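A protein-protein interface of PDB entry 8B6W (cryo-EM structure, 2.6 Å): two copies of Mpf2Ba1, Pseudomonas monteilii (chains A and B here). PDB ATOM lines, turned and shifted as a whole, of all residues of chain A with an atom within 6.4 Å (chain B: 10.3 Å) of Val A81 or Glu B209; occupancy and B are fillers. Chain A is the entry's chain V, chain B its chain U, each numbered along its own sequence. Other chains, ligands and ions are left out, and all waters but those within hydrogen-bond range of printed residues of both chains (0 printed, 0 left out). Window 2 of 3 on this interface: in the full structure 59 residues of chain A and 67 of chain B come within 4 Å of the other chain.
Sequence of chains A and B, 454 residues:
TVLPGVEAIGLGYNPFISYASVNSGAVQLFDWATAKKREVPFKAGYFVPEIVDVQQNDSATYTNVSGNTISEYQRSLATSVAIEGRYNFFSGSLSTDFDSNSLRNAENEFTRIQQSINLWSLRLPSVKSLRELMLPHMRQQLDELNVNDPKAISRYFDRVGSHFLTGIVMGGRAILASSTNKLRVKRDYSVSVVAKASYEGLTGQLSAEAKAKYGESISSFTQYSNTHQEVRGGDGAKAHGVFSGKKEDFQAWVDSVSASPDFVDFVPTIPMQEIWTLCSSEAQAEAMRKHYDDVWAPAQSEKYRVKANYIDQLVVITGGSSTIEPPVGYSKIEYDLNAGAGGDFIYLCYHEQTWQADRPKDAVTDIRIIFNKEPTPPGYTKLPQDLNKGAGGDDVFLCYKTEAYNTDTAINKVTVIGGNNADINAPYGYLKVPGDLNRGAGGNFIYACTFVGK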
ATOM      1  N   THR A  79       2.974  28.162 -21.350  1.00  0.00           N
ATOM      2  CA  THR A  79       3.250  26.976 -22.146  1.00  0.00           C
ATOM      3  C   THR A  79       3.315  27.379 -23.609  1.00  0.00           C
ATOM      4  O   THR A  79       2.570  28.258 -24.046  1.00  0.00           O
ATOM      5  CB  THR A  79       2.182  25.898 -21.938  1.00  0.00           C
ATOM      6  OG1 THR A  79       2.347  25.306 -20.644  1.00  0.00           O
ATOM      7  CG2 THR A  79       2.294  24.821 -23.004  1.00  0.00           C
ATOM      8  N   SER A  80       4.216  26.752 -24.359  1.00  0.00           N
ATOM      9  CA  SER A  80       4.249  26.927 -25.804  1.00  0.00           C
ATOM     10  C   SER A  80       4.660  25.626 -26.472  1.00  0.00           C
ATOM     11  O   SER A  80       5.488  24.881 -25.943  1.00  0.00           O
ATOM     12  CB  SER A  80       5.217  28.045 -26.203  1.00  0.00           C
ATOM     13  OG  SER A  80       4.886  29.257 -25.552  1.00  0.00           O
ATOM     14  N   VAL A  81       4.056  25.354 -27.624  1.00  0.00           N
ATOM     15  CA  VAL A  81       4.392  24.203 -28.454  1.00  0.00           C
ATOM     16  C   VAL A  81       4.450  24.678 -29.897  1.00  0.00           C
ATOM     17  O   VAL A  81       3.591  25.445 -30.340  1.00  0.00           O
ATOM     18  CB  VAL A  81       3.371  23.061 -28.291  1.00  0.00           C
ATOM     19  CG1 VAL A  81       3.646  21.960 -29.297  1.00  0.00           C
ATOM     20  CG2 VAL A  81       3.409  22.519 -26.875  1.00  0.00           C
ATOM     21  N   ALA A  82       5.470  24.239 -30.628  1.00  0.00           N
ATOM     22  CA  ALA A  82       5.537  24.459 -32.066  1.00  0.00           C
ATOM     23  C   ALA A  82       5.923  23.171 -32.773  1.00  0.00           C
ATOM     24  O   ALA A  82       6.837  22.464 -32.335  1.00  0.00           O
ATOM     25  CB  ALA A  82       6.541  25.565 -32.406  1.00  0.00           C
ATOM     26  N   ILE A  83       5.219  22.865 -33.858  1.00  0.00           N
ATOM     27  CA  ILE A  83       5.387  21.626 -34.603  1.00  0.00           C
ATOM     28  C   ILE A  83       5.535  21.993 -36.071  1.00  0.00           C
ATOM     29  O   ILE A  83       4.905  22.944 -36.543  1.00  0.00           O
ATOM     30  CB  ILE A  83       4.197  20.666 -34.403  1.00  0.00           C
ATOM     31  CG1 ILE A  83       4.027  20.314 -32.925  1.00  0.00           C
ATOM     32  CG2 ILE A  83       4.383  19.411 -35.235  1.00  0.00           C
ATOM     33  CD1 ILE A  83       5.159  19.499 -32.346  1.00  0.00           C
ATOM     34  N   LEU A  94       1.941  23.725 -36.925  1.00  0.00           N
ATOM     35  CA  LEU A  94       0.996  23.891 -35.833  1.00  0.00           C
ATOM     36  C   LEU A  94       1.678  24.656 -34.711  1.00  0.00           C
ATOM     37  O   LEU A  94       2.859  24.440 -34.433  1.00  0.00           O
ATOM     38  CB  LEU A  94       0.481  22.537 -35.329  1.00  0.00           C
ATOM     39  CG  LEU A  94      -0.421  22.558 -34.096  1.00  0.00           C
ATOM     40  CD1 LEU A  94      -1.395  21.392 -34.152  1.00  0.00           C
ATOM     41  CD2 LEU A  94       0.377  22.512 -32.804  1.00  0.00           C
ATOM     42  N   SER A  95       0.931  25.553 -34.076  1.00  0.00           N
ATOM     43  CA  SER A  95       1.378  26.237 -32.873  1.00  0.00           C
ATOM     44  C   SER A  95       0.291  26.141 -31.814  1.00  0.00           C
ATOM     45  O   SER A  95      -0.899  26.177 -32.131  1.00  0.00           O
ATOM     46  CB  SER A  95       1.707  27.707 -33.151  1.00  0.00           C
ATOM     47  OG  SER A  95       2.097  28.371 -31.963  1.00  0.00           O
ATOM     48  N   THR A  96       0.706  26.006 -30.560  1.00  0.00           N
ATOM     49  CA  THR A  96      -0.208  26.109 -29.433  1.00  0.00           C
ATOM     50  C   THR A  96       0.449  26.915 -28.325  1.00  0.00           C
ATOM     51  O   THR A  96       1.631  26.727 -28.026  1.00  0.00           O
ATOM     52  CB  THR A  96      -0.606  24.730 -28.906  1.00  0.00           C
ATOM     53  OG1 THR A  96      -1.354  24.031 -29.910  1.00  0.00           O
ATOM     54  CG2 THR A  96      -1.450  24.861 -27.650  1.00  0.00           C
ATOM     55  N   ASP A  97      -0.324  27.814 -27.727  1.00  0.00           N
ATOM     56  CA  ASP A  97       0.166  28.696 -26.681  1.00  0.00           C
ATOM     57  C   ASP A  97      -0.886  28.753 -25.588  1.00  0.00           C
ATOM     58  O   ASP A  97      -2.077  28.882 -25.878  1.00  0.00           O
ATOM     59  CB  ASP A  97       0.460  30.096 -27.231  1.00  0.00           C
ATOM     60  CG  ASP A  97       0.914  31.068 -26.159  1.00  0.00           C
ATOM     61  OD1 ASP A  97       0.706  30.797 -24.959  1.00  0.00           O
ATOM     62  OD2 ASP A  97       1.485  32.116 -26.525  1.00  0.00           O
ATOM     63  N   SER B  91      19.017  17.036 -34.671  1.00  0.00           N
ATOM     64  CA  SER B  91      19.560  17.936 -33.667  1.00  0.00           C
ATOM     65  C   SER B  91      18.596  18.026 -32.494  1.00  0.00           C
ATOM     66  O   SER B  91      17.382  18.134 -32.686  1.00  0.00           O
ATOM     67  CB  SER B  91      19.801  19.333 -34.250  1.00  0.00           C
ATOM     68  OG  SER B  91      20.307  20.214 -33.264  1.00  0.00           O
ATOM     69  N   GLY B  92      19.138  17.969 -31.292  1.00  0.00           N
ATOM     70  CA  GLY B  92      18.335  18.094 -30.085  1.00  0.00           C
ATOM     71  C   GLY B  92      18.919  19.128 -29.150  1.00  0.00           C
ATOM     72  O   GLY B  92      20.135  19.242 -29.014  1.00  0.00           O
ATOM     73  N   SER B  93      18.035  19.890 -28.512  1.00  0.00           N
ATOM     74  CA  SER B  93      18.430  20.840 -27.485  1.00  0.00           C
ATOM     75  C   SER B  93      17.465  20.747 -26.315  1.00  0.00           C
ATOM     76  O   SER B  93      16.260  20.572 -26.509  1.00  0.00           O
ATOM     77  CB  SER B  93      18.460  22.273 -28.022  1.00  0.00           C
ATOM     78  OG  SER B  93      18.677  23.202 -26.977  1.00  0.00           O
ATOM     79  N   LEU B  94      18.001  20.848 -25.103  1.00  0.00           N
ATOM     80  CA  LEU B  94      17.187  20.977 -23.906  1.00  0.00           C
ATOM     81  C   LEU B  94      17.811  22.028 -23.006  1.00  0.00           C
ATOM     82  O   LEU B  94      19.036  22.110 -22.891  1.00  0.00           O
ATOM     83  CB  LEU B  94      17.064  19.637 -23.168  1.00  0.00           C
ATOM     84  CG  LEU B  94      16.342  19.656 -21.821  1.00  0.00           C
ATOM     85  CD1 LEU B  94      15.663  18.318 -21.583  1.00  0.00           C
ATOM     86  CD2 LEU B  94      17.286  19.976 -20.674  1.00  0.00           C
ATOM     87  N   SER B  95      16.965  22.836 -22.375  1.00  0.00           N
ATOM     88  CA  SER B  95      17.389  23.775 -21.348  1.00  0.00           C
ATOM     89  C   SER B  95      16.495  23.616 -20.128  1.00  0.00           C
ATOM     90  O   SER B  95      15.299  23.353 -20.258  1.00  0.00           O
ATOM     91  CB  SER B  95      17.337  25.220 -21.849  1.00  0.00           C
ATOM     92  OG  SER B  95      17.710  26.125 -20.826  1.00  0.00           O
ATOM     93  N   SER B 192      11.857  27.397 -15.587  1.00  0.00           N
ATOM     94  CA  SER B 192      11.748  27.503 -17.032  1.00  0.00           C
ATOM     95  C   SER B 192      12.343  26.263 -17.679  1.00  0.00           C
ATOM     96  O   SER B 192      13.408  25.791 -17.274  1.00  0.00           O
ATOM     97  CB  SER B 192      12.459  28.755 -17.549  1.00  0.00           C
ATOM     98  OG  SER B 192      12.451  28.797 -18.963  1.00  0.00           O
ATOM     99  N   VAL B 193      11.643  25.732 -18.676  1.00  0.00           N
ATOM    100  CA  VAL B 193      12.050  24.520 -19.372  1.00  0.00           C
ATOM    101  C   VAL B 193      11.867  24.740 -20.864  1.00  0.00           C
ATOM    102  O   VAL B 193      10.844  25.274 -21.302  1.00  0.00           O
ATOM    103  CB  VAL B 193      11.239  23.297 -18.898  1.00  0.00           C
ATOM    104  CG1 VAL B 193      11.660  22.055 -19.663  1.00  0.00           C
ATOM    105  CG2 VAL B 193      11.412  23.101 -17.402  1.00  0.00           C
ATOM    106  N   VAL B 194      12.862  24.334 -21.646  1.00  0.00           N
ATOM    107  CA  VAL B 194      12.789  24.366 -23.100  1.00  0.00           C
ATOM    108  C   VAL B 194      13.258  23.018 -23.629  1.00  0.00           C
ATOM    109  O   VAL B 194      14.280  22.494 -23.177  1.00  0.00           O
ATOM    110  CB  VAL B 194      13.643  25.502 -23.692  1.00  0.00           C
ATOM    111  CG1 VAL B 194      13.486  25.551 -25.200  1.00  0.00           C
ATOM    112  CG2 VAL B 194      13.267  26.840 -23.068  1.00  0.00           C
ATOM    113  N   ALA B 195      12.510  22.462 -24.577  1.00  0.00           N
ATOM    114  CA  ALA B 195      12.912  21.257 -25.288  1.00  0.00           C
ATOM    115  C   ALA B 195      12.689  21.458 -26.776  1.00  0.00           C
ATOM    116  O   ALA B 195      11.612  21.894 -27.190  1.00  0.00           O
ATOM    117  CB  ALA B 195      12.130  20.039 -24.793  1.00  0.00           C
ATOM    118  N   LYS B 196      13.705  21.148 -27.575  1.00  0.00           N
ATOM    119  CA  LYS B 196      13.670  21.382 -29.010  1.00  0.00           C
ATOM    120  C   LYS B 196      14.200  20.153 -29.732  1.00  0.00           C
ATOM    121  O   LYS B 196      15.171  19.538 -29.286  1.00  0.00           O
ATOM    122  CB  LYS B 196      14.489  22.620 -29.383  1.00  0.00           C
ATOM    123  CG  LYS B 196      14.370  23.023 -30.839  1.00  0.00           C
ATOM    124  CD  LYS B 196      15.295  24.182 -31.182  1.00  0.00           C
ATOM    125  CE  LYS B 196      14.998  25.415 -30.340  1.00  0.00           C
ATOM    126  NZ  LYS B 196      15.848  26.573 -30.723  1.00  0.00           N
ATOM    127  N   ALA B 197      13.552  19.792 -30.839  1.00  0.00           N
ATOM    128  CA  ALA B 197      14.014  18.700 -31.683  1.00  0.00           C
ATOM    129  C   ALA B 197      13.939  19.114 -33.145  1.00  0.00           C
ATOM    130  O   ALA B 197      12.995  19.790 -33.559  1.00  0.00           O
ATOM    131  CB  ALA B 197      13.183  17.431 -31.459  1.00  0.00           C
ATOM    132  N   SER B 198      14.943  18.709 -33.919  1.00  0.00           N
ATOM    133  CA  SER B 198      14.943  18.858 -35.370  1.00  0.00           C
ATOM    134  C   SER B 198      15.372  17.544 -36.001  1.00  0.00           C
ATOM    135  O   SER B 198      16.336  16.923 -35.546  1.00  0.00           O
ATOM    136  CB  SER B 198      15.877  19.988 -35.811  1.00  0.00           C
ATOM    137  OG  SER B 198      15.912  20.094 -37.222  1.00  0.00           O
ATOM    138  N   TYR B 199      14.656  17.118 -37.041  1.00  0.00           N
ATOM    139  CA  TYR B 199      14.819  15.780 -37.591  1.00  0.00           C
ATOM    140  C   TYR B 199      14.639  15.827 -39.100  1.00  0.00           C
ATOM    141  O   TYR B 199      13.831  16.606 -39.612  1.00  0.00           O
ATOM    142  CB  TYR B 199      13.809  14.808 -36.966  1.00  0.00           C
ATOM    143  CG  TYR B 199      13.811  13.423 -37.570  1.00  0.00           C
ATOM    144  CD1 TYR B 199      12.965  13.102 -38.624  1.00  0.00           C
ATOM    145  CD2 TYR B 199      14.648  12.431 -37.077  1.00  0.00           C
ATOM    146  CE1 TYR B 199      12.951  11.831 -39.167  1.00  0.00           C
ATOM    147  CE2 TYR B 199      14.647  11.157 -37.621  1.00  0.00           C
ATOM    148  CZ  TYR B 199      13.794  10.864 -38.665  1.00  0.00           C
ATOM    149  OH  TYR B 199      13.796   9.605 -39.219  1.00  0.00           O
ATOM    150  N   LEU B 206      10.936  17.838 -40.029  1.00  0.00           N
ATOM    151  CA  LEU B 206      10.113  17.988 -38.844  1.00  0.00           C
ATOM    152  C   LEU B 206      10.835  18.917 -37.885  1.00  0.00           C
ATOM    153  O   LEU B 206      12.056  18.826 -37.726  1.00  0.00           O
ATOM    154  CB  LEU B 206       9.841  16.634 -38.180  1.00  0.00           C
ATOM    155  CG  LEU B 206       9.131  16.658 -36.827  1.00  0.00           C
ATOM    156  CD1 LEU B 206       7.724  17.205 -36.970  1.00  0.00           C
ATOM    157  CD2 LEU B 206       9.104  15.265 -36.221  1.00  0.00           C
ATOM    158  N   SER B 207      10.085  19.811 -37.261  1.00  0.00           N
ATOM    159  CA  SER B 207      10.556  20.535 -36.094  1.00  0.00           C
ATOM    160  C   SER B 207       9.498  20.452 -35.009  1.00  0.00           C
ATOM    161  O   SER B 207       8.300  20.540 -35.287  1.00  0.00           O
ATOM    162  CB  SER B 207      10.856  22.001 -36.424  1.00  0.00           C
ATOM    163  OG  SER B 207      11.189  22.724 -35.253  1.00  0.00           O
ATOM    164  N   ALA B 208       9.947  20.273 -33.775  1.00  0.00           N
ATOM    165  CA  ALA B 208       9.057  20.245 -32.629  1.00  0.00           C
ATOM    166  C   ALA B 208       9.681  21.075 -31.526  1.00  0.00           C
ATOM    167  O   ALA B 208      10.905  21.098 -31.371  1.00  0.00           O
ATOM    168  CB  ALA B 208       8.803  18.815 -32.141  1.00  0.00           C
ATOM    169  N   GLU B 209       8.840  21.772 -30.773  1.00  0.00           N
ATOM    170  CA  GLU B 209       9.281  22.488 -29.592  1.00  0.00           C
ATOM    171  C   GLU B 209       8.233  22.362 -28.503  1.00  0.00           C
ATOM    172  O   GLU B 209       7.033  22.336 -28.783  1.00  0.00           O
ATOM    173  CB  GLU B 209       9.537  23.965 -29.894  1.00  0.00           C
ATOM    174  CG  GLU B 209       9.990  24.754 -28.688  1.00  0.00           C
ATOM    175  CD  GLU B 209      10.452  26.139 -29.054  1.00  0.00           C
ATOM    176  OE1 GLU B 209      11.120  26.282 -30.097  1.00  0.00           O
ATOM    177  OE2 GLU B 209      10.153  27.087 -28.297  1.00  0.00           O
ATOM    178  N   ALA B 210       8.696  22.273 -27.265  1.00  0.00           N
ATOM    179  CA  ALA B 210       7.845  22.444 -26.104  1.00  0.00           C
ATOM    180  C   ALA B 210       8.504  23.443 -25.173  1.00  0.00           C
ATOM    181  O   ALA B 210       9.729  23.445 -25.021  1.00  0.00           O
ATOM    182  CB  ALA B 210       7.608  21.118 -25.375  1.00  0.00           C
ATOM    183  N   LYS B 211       7.696  24.297 -24.563  1.00  0.00           N
ATOM    184  CA  LYS B 211       8.187  25.263 -23.598  1.00  0.00           C
ATOM    185  C   LYS B 211       7.237  25.286 -22.419  1.00  0.00           C
ATOM    186  O   LYS B 211       6.020  25.179 -22.591  1.00  0.00           O
ATOM    187  CB  LYS B 211       8.305  26.655 -24.221  1.00  0.00           C
ATOM    188  CG  LYS B 211       8.939  27.688 -23.312  1.00  0.00           C
ATOM    189  CD  LYS B 211       9.179  29.013 -24.023  1.00  0.00           C
ATOM    190  CE  LYS B 211      10.145  28.881 -25.190  1.00  0.00           C
ATOM    191  NZ  LYS B 211      10.452  30.201 -25.805  1.00  0.00           N
ATOM    192  N   ALA B 212       7.792  25.411 -21.222  1.00  0.00           N
ATOM    193  CA  ALA B 212       6.998  25.622 -20.028  1.00  0.00           C
ATOM    194  C   ALA B 212       7.710  26.615 -19.132  1.00  0.00           C
ATOM    195  O   ALA B 212       8.936  26.592 -19.016  1.00  0.00           O
ATOM    196  CB  ALA B 212       6.750  24.313 -19.273  1.00  0.00           C
ATOM    197  N   LYS B 213       6.936  27.489 -18.510  1.00  0.00           N
ATOM    198  CA  LYS B 213       7.417  28.363 -17.456  1.00  0.00           C
ATOM    199  C   LYS B 213       6.431  28.326 -16.305  1.00  0.00           C
ATOM    200  O   LYS B 213       5.220  28.216 -16.515  1.00  0.00           O
ATOM    201  CB  LYS B 213       7.633  29.802 -17.923  1.00  0.00           C
ATOM    202  CG  LYS B 213       8.324  30.633 -16.859  1.00  0.00           C
ATOM    203  CD  LYS B 213       8.462  32.094 -17.223  1.00  0.00           C
ATOM    204  CE  LYS B 213       9.430  32.301 -18.368  1.00  0.00           C
ATOM    205  NZ  LYS B 213       9.591  33.747 -18.676  1.00  0.00           N
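The backbone NH of Glu B209 sits at hydrogen-bond distance from the backbone carbonyl oxygen of Ala A82, at 2.6 Å.
O of Ser A80 is in hydrogen-bond range of N of Lys B211 (2.7 Å).
The backbone NH (N) of Ala B210 lies within hydrogen-bond range of the backbone carbonyl oxygen (O) of Ala B195 (2.9 Å).
The backbone NH (N) of Ala B197 is in hydrogen-bond range of the backbone carbonyl oxygen (O) of Ala B208 (3.0 Å).
The side-chain carboxylate (OE2) of Glu B209 lies within salt-bridge range of the side-chain amino group (NZ) of Lys B211 (3.9996 Å).
The backbone carbonyl oxygen (O) of Thr A96 sits at hydrogen-bond distance from the backbone NH (N) of Val A81, 2.8 Å away.
N of Ile A83 is in hydrogen-bond range of O of Leu A94 (2.9 Å).
Among the printed residues, pairs that only touch across the chains: Ala A82 with Ala B208 (3.2 Å), Ile A83 with Ser B207 (3.2 Å), Val A81 with Glu B209 (3.3 Å), Thr A79 with Lys B211 (3.3 Å), Ser A80 with Ala B210 (3.4 Å), Ile A83 with Ala B208 (3.7 Å) and Ala A82 with Ser B207 (3.8 Å).
Glu B209 touches two residues of chain A.
Of chain B, only Ala B210 (3.4 Å) and Lys B211 (2.7 Å) come within 4 Å of Ser A80.
Ala A82 touches just these residues of chain B: Ser B207 (3.8 Å), Ala B208 (3.2 Å) and Glu B209 (2.6 Å).
No residue of chain B comes within 4 Å of Ser A95.
No residue of chain B comes within 4 Å of Thr A96.
Of the printed residues of chain A, Ala B208 touches Ala A82 and Ile A83.
Printed residues of chain B within 4 Å of Thr A79: Lys B211 (3.3 Å).
Of the printed residues of chain A, Ala B210 touches Ser A80.
The nearest residue of chain B that does not touch Val A81 is Ala B210 (4.5 Å).
The nearest residue of chain A that does not touch Glu B209 is Ser A80 (4.1 Å).
The nearest printed residue of chain B that does not touch Thr A79 is Ala B212 (4.5 Å).
Of the 21 printed residues of chain B, 5 touch a printed residue of chain A.
Along chain B the printed residues that touch a printed residue of chain A span positions 207 to 211.
Printed residues of chain A that touch a printed residue of chain B: Thr A79, Ser A80, Val A81, Ala A82 and Ile A83.
Hydrophobic or aromatic side chains of chain A that line the printed part of chain B: Val A81 and Ile A83.
Among the printed residues, 9 pairs touch across the chains.
2 positions are printed for both chains.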
